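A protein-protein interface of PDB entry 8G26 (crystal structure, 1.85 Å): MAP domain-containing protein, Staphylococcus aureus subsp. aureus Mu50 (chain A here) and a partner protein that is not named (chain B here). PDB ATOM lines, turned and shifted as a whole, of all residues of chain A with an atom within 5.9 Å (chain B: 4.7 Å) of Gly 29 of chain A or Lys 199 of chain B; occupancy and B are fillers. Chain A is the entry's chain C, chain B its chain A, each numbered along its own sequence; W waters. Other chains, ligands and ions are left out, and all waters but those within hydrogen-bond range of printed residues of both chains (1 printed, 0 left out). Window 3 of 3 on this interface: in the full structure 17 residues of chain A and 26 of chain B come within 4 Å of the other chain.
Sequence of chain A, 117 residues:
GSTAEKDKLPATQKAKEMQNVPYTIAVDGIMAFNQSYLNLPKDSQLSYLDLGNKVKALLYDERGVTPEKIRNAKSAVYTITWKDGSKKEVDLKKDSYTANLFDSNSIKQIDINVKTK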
ATOM      1  N   ALA A  26      31.987  24.423   5.834  1.00  0.00           N
ATOM      2  CA  ALA A  26      31.007  23.405   5.482  1.00  0.00           C
ATOM      3  C   ALA A  26      31.763  22.110   5.231  1.00  0.00           C
ATOM      4  O   ALA A  26      32.778  22.113   4.526  1.00  0.00           O
ATOM      5  CB  ALA A  26      30.191  23.828   4.254  1.00  0.00           C
ATOM      6  N   VAL A  27      31.319  21.033   5.878  1.00  0.00           N
ATOM      7  CA  VAL A  27      31.866  19.698   5.682  1.00  0.00           C
ATOM      8  C   VAL A  27      30.706  18.760   5.373  1.00  0.00           C
ATOM      9  O   VAL A  27      29.763  18.661   6.164  1.00  0.00           O
ATOM     10  CB  VAL A  27      32.623  19.177   6.922  1.00  0.00           C
ATOM     11  CG1 VAL A  27      33.270  17.815   6.594  1.00  0.00           C
ATOM     12  CG2 VAL A  27      33.632  20.165   7.391  1.00  0.00           C
ATOM     13  N   ASP A  28      30.785  18.057   4.245  1.00  0.00           N
ATOM     14  CA  ASP A  28      29.735  17.119   3.845  1.00  0.00           C
ATOM     15  C   ASP A  28      28.360  17.787   3.875  1.00  0.00           C
ATOM     16  O   ASP A  28      27.361  17.186   4.276  1.00  0.00           O
ATOM     17  CB  ASP A  28      29.760  15.874   4.732  1.00  0.00           C
ATOM     18  CG  ASP A  28      31.023  15.056   4.541  1.00  0.00           C
ATOM     19  OD1 ASP A  28      31.410  14.847   3.368  1.00  0.00           O
ATOM     20  OD2 ASP A  28      31.632  14.637   5.556  1.00  0.00           O
ATOM     21  N   GLY A  29      28.314  19.049   3.447  1.00  0.00           N
ATOM     22  CA  GLY A  29      27.063  19.777   3.365  1.00  0.00           C
ATOM     23  C   GLY A  29      26.446  20.191   4.683  1.00  0.00           C
ATOM     24  O   GLY A  29      25.245  20.459   4.731  1.00  0.00           O
ATOM     25  N   ILE A  30      27.219  20.229   5.764  1.00  0.00           N
ATOM     26  CA  ILE A  30      26.743  20.675   7.062  1.00  0.00           C
ATOM     27  C   ILE A  30      27.561  21.904   7.450  1.00  0.00           C
ATOM     28  O   ILE A  30      28.797  21.873   7.414  1.00  0.00           O
ATOM     29  CB  ILE A  30      26.883  19.576   8.130  1.00  0.00           C
ATOM     30  CG1 ILE A  30      25.807  18.500   8.007  1.00  0.00           C
ATOM     31  CG2 ILE A  30      26.805  20.191   9.529  1.00  0.00           C
ATOM     32  CD1 ILE A  30      25.742  17.793   6.642  1.00  0.00           C
ATOM     33  N   MET A  31      26.874  22.981   7.823  1.00  0.00           N
ATOM     34  CA  MET A  31      27.531  24.178   8.331  1.00  0.00           C
ATOM     35  C   MET A  31      26.893  24.561   9.659  1.00  0.00           C
ATOM     36  O   MET A  31      25.683  24.746   9.718  1.00  0.00           O
ATOM     37  CB  MET A  31      27.402  25.334   7.323  1.00  0.00           C
ATOM     38  CG  MET A  31      27.974  26.669   7.812  1.00  0.00           C
ATOM     39  SD  MET A  31      27.781  27.971   6.540  1.00  0.00           S
ATOM     40  CE  MET A  31      26.068  28.393   6.814  1.00  0.00           C
ATOM     41  N   PHE A  33      25.711  27.029  12.540  1.00  0.00           N
ATOM     42  CA  PHE A  33      25.134  28.360  12.392  1.00  0.00           C
ATOM     43  C   PHE A  33      25.659  29.377  13.419  1.00  0.00           C
ATOM     44  O   PHE A  33      24.931  30.290  13.808  1.00  0.00           O
ATOM     45  CB  PHE A  33      23.609  28.248  12.437  1.00  0.00           C
ATOM     46  CG  PHE A  33      22.992  27.752  11.134  1.00  0.00           C
ATOM     47  CD1 PHE A  33      23.742  27.712   9.959  1.00  0.00           C
ATOM     48  CD2 PHE A  33      21.673  27.351  11.081  1.00  0.00           C
ATOM     49  CE1 PHE A  33      23.186  27.264   8.768  1.00  0.00           C
ATOM     50  CE2 PHE A  33      21.099  26.914   9.873  1.00  0.00           C
ATOM     51  CZ  PHE A  33      21.859  26.887   8.720  1.00  0.00           C
ATOM     52  N   VAL A 114      34.708  21.271   2.483  1.00  0.00           N
ATOM     53  CA  VAL A 114      35.297  19.943   2.408  1.00  0.00           C
ATOM     54  C   VAL A 114      34.197  18.947   2.070  1.00  0.00           C
ATOM     55  O   VAL A 114      33.160  18.910   2.737  1.00  0.00           O
ATOM     56  CB  VAL A 114      35.991  19.551   3.723  1.00  0.00           C
ATOM     57  CG1 VAL A 114      36.409  18.094   3.665  1.00  0.00           C
ATOM     58  CG2 VAL A 114      37.197  20.457   3.996  1.00  0.00           C
ATOM     59  N   LYS A 115      34.430  18.124   1.056  1.00  0.00           N
ATOM     60  CA  LYS A 115      33.478  17.085   0.681  1.00  0.00           C
ATOM     61  C   LYS A 115      34.180  15.740   0.623  1.00  0.00           C
ATOM     62  O   LYS A 115      35.163  15.584  -0.105  1.00  0.00           O
ATOM     63  CB  LYS A 115      32.821  17.422  -0.658  1.00  0.00           C
ATOM     64  CG  LYS A 115      31.724  18.456  -0.507  1.00  0.00           C
ATOM     65  CD  LYS A 115      31.918  19.636  -1.435  1.00  0.00           C
ATOM     66  CE  LYS A 115      30.679  20.524  -1.435  1.00  0.00           C
ATOM     67  NZ  LYS A 115      29.521  19.866  -2.106  1.00  0.00           N
ATOM     68  N   ILE B 155      19.311  14.465   3.558  1.00  0.00           N
ATOM     69  CA  ILE B 155      20.197  15.601   3.304  1.00  0.00           C
ATOM     70  C   ILE B 155      21.395  15.615   4.243  1.00  0.00           C
ATOM     71  O   ILE B 155      22.491  16.016   3.864  1.00  0.00           O
ATOM     72  CB  ILE B 155      19.410  16.918   3.446  1.00  0.00           C
ATOM     73  CG1 ILE B 155      18.329  17.076   2.382  1.00  0.00           C
ATOM     74  CG2 ILE B 155      20.387  18.086   3.401  1.00  0.00           C
ATOM     75  CD1 ILE B 155      17.341  18.191   2.747  1.00  0.00           C
ATOM     76  N   PHE B 156      21.178  15.251   5.493  1.00  0.00           N
ATOM     77  CA  PHE B 156      22.172  15.348   6.561  1.00  0.00           C
ATOM     78  C   PHE B 156      22.440  13.920   7.025  1.00  0.00           C
ATOM     79  O   PHE B 156      21.692  13.383   7.853  1.00  0.00           O
ATOM     80  CB  PHE B 156      21.672  16.231   7.710  1.00  0.00           C
ATOM     81  CG  PHE B 156      21.273  17.639   7.300  1.00  0.00           C
ATOM     82  CD1 PHE B 156      22.228  18.559   6.871  1.00  0.00           C
ATOM     83  CD2 PHE B 156      19.958  18.050   7.376  1.00  0.00           C
ATOM     84  CE1 PHE B 156      21.861  19.849   6.508  1.00  0.00           C
ATOM     85  CE2 PHE B 156      19.592  19.341   7.011  1.00  0.00           C
ATOM     86  CZ  PHE B 156      20.538  20.234   6.584  1.00  0.00           C
ATOM     87  N   PHE B 177      19.895  31.146  10.669  1.00  0.00           N
ATOM     88  CA  PHE B 177      21.096  31.254   9.839  1.00  0.00           C
ATOM     89  C   PHE B 177      22.269  31.677  10.724  1.00  0.00           C
ATOM     90  O   PHE B 177      22.212  31.567  11.953  1.00  0.00           O
ATOM     91  CB  PHE B 177      20.779  32.179   8.650  1.00  0.00           C
ATOM     92  CG  PHE B 177      21.733  32.045   7.482  1.00  0.00           C
ATOM     93  CD1 PHE B 177      22.139  30.801   7.025  1.00  0.00           C
ATOM     94  CD2 PHE B 177      22.213  33.182   6.845  1.00  0.00           C
ATOM     95  CE1 PHE B 177      23.014  30.699   5.973  1.00  0.00           C
ATOM     96  CE2 PHE B 177      23.078  33.072   5.791  1.00  0.00           C
ATOM     97  CZ  PHE B 177      23.473  31.831   5.355  1.00  0.00           C
ATOM     98  N   GLY B 198      22.791  23.732   9.439  1.00  0.00           N
ATOM     99  CA  GLY B 198      22.050  23.553   8.211  1.00  0.00           C
ATOM    100  C   GLY B 198      22.975  23.631   7.013  1.00  0.00           C
ATOM    101  O   GLY B 198      24.169  23.379   7.107  1.00  0.00           O
ATOM    102  N   LYS B 199      22.382  23.989   5.872  1.00  0.00           N
ATOM    103  CA  LYS B 199      23.148  24.150   4.633  1.00  0.00           C
ATOM    104  C   LYS B 199      23.775  25.528   4.547  1.00  0.00           C
ATOM    105  O   LYS B 199      23.218  26.513   5.030  1.00  0.00           O
ATOM    106  CB  LYS B 199      22.240  23.933   3.431  1.00  0.00           C
ATOM    107  CG  LYS B 199      21.832  22.493   3.222  1.00  0.00           C
ATOM    108  CD  LYS B 199      22.969  21.751   2.553  1.00  0.00           C
ATOM    109  CE  LYS B 199      22.811  20.243   2.626  1.00  0.00           C
ATOM    110  NZ  LYS B 199      23.866  19.579   1.792  1.00  0.00           N
ATOM    111  N   SER B 200      24.939  25.597   3.871  1.00  0.00           N
ATOM    112  CA  SER B 200      25.610  26.876   3.693  1.00  0.00           C
ATOM    113  C   SER B 200      24.700  27.889   3.014  1.00  0.00           C
ATOM    114  O   SER B 200      24.818  29.098   3.261  1.00  0.00           O
ATOM    115  CB  SER B 200      26.874  26.674   2.858  1.00  0.00           C
ATOM    116  OG  SER B 200      26.492  26.389   1.533  1.00  0.00           O
ATOM    117  N   SER B 201      23.818  27.420   2.142  1.00  0.00           N
ATOM    118  CA  SER B 201      22.875  28.283   1.451  1.00  0.00           C
ATOM    119  C   SER B 201      21.811  28.878   2.367  1.00  0.00           C
ATOM    120  O   SER B 201      21.161  29.852   1.984  1.00  0.00           O
ATOM    121  CB  SER B 201      22.170  27.475   0.371  1.00  0.00           C
ATOM    122  OG  SER B 201      21.375  26.467   1.012  1.00  0.00           O
ATOM    123  N   GLY B 202      21.565  28.276   3.532  1.00  0.00           N
ATOM    124  CA  GLY B 202      20.445  28.674   4.364  1.00  0.00           C
ATOM    125  C   GLY B 202      19.091  28.136   3.946  1.00  0.00           C
ATOM    126  O   GLY B 202      18.080  28.443   4.603  1.00  0.00           O
ATOM    127  N   VAL B 203      19.026  27.313   2.909  1.00  0.00           N
ATOM    128  CA  VAL B 203      17.741  26.739   2.484  1.00  0.00           C
ATOM    129  C   VAL B 203      17.298  25.693   3.498  1.00  0.00           C
ATOM    130  O   VAL B 203      18.134  24.886   3.937  1.00  0.00           O
ATOM    131  CB  VAL B 203      17.874  26.123   1.091  1.00  0.00           C
ATOM    132  CG1 VAL B 203      16.530  25.580   0.639  1.00  0.00           C
ATOM    133  CG2 VAL B 203      18.427  27.157   0.069  1.00  0.00           C
HETATM  134  O   HOH W   1      26.220  23.127   3.149  1.00  0.00           O
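O of Gly 198 of chain B is in hydrogen-bond range of N of Met 31 of chain A (2.8 Å).
The side-chain amino group (NZ) of Lys 199 of chain B sits close to the backbone carbonyl oxygen (O) of Gly 29 of chain A, at 3.4 Å.
Printed residues of chain B within 4 Å of Gly 29 of chain A: Phe 156 (3.9 Å), Gly 198 (3.9 Å) and Lys 199 (3.2 Å).
Lys 199 of chain B touches just these residues of chain A: Gly 29, Met 31 and Phe 33.
Printed residues of chain B within 4 Å of Phe 33 of chain A: Phe 177 (3.5 Å), Gly 198 (3.4 Å) and Lys 199 (3.8 Å).
Printed residues of chain A within 4 Å of Gly 198 of chain B: Gly 29, Ile 30, Met 31 and Phe 33.
Of the printed residues of chain B, Met 31 of chain A touches Phe 177, Gly 198, Lys 199 and Ser 200.
Ala 26 of chain A touches none of the printed residues of chain B.
Val 114 of chain A touches none of the printed residues of chain B.
The nearest printed residue of chain B that does not touch Gly 29 of chain A is Ser 200 of chain B (5.2 Å).
Water W1 lies within hydrogen-bond range of N of Ser 200 of chain B (2.9 Å) and O of Gly 29 of chain A (3.3 Å).
CE1 of Phe 156 of chain B touches O of Gly 29 of chain A, 3.9 Å away.
O of Gly 198 of chain B touches O of Gly 29 of chain A (3.9 Å).
CD1 of Ile 30 of chain A touches CD1 of Phe 156 of chain B (3.6 Å).
Gly 198 of chain B touches Ile 30 of chain A (O to C, 3.7 Å).
Phe 177 of chain B touches Met 31 of chain A.
CE of Met 31 of chain A touches O of Lys 199 of chain B (3.9 Å).
Ser 200 of chain B touches Met 31 of chain A (CA to CE, 3.5 Å).
O of Phe 33 of chain A touches O of Phe 177 of chain B, at 3.5 Å.
Phe 33 of chain A touches Gly 198 of chain B (CZ to N, 3.4 Å).
Lys 199 of chain B touches Phe 33 of chain A (O to CE1, 3.8 Å).
Of the 9 printed residues of chain A, 4 touch a printed residue of chain B.
Hydrophobic or aromatic side chains of chain A that line the printed part of chain B: Ile 30, Met 31 and Phe 33.
Of the 9 printed residues of chain B, 5 touch a printed residue of chain A.
Hydrophobic or aromatic side chains of chain B within 4 Å of the printed part of chain A: Phe 156 and Phe 177.
Along chain B the printed residues that touch a printed residue of chain A span positions 156 to 200.
Among the printed residues, 12 pairs touch across the chains.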
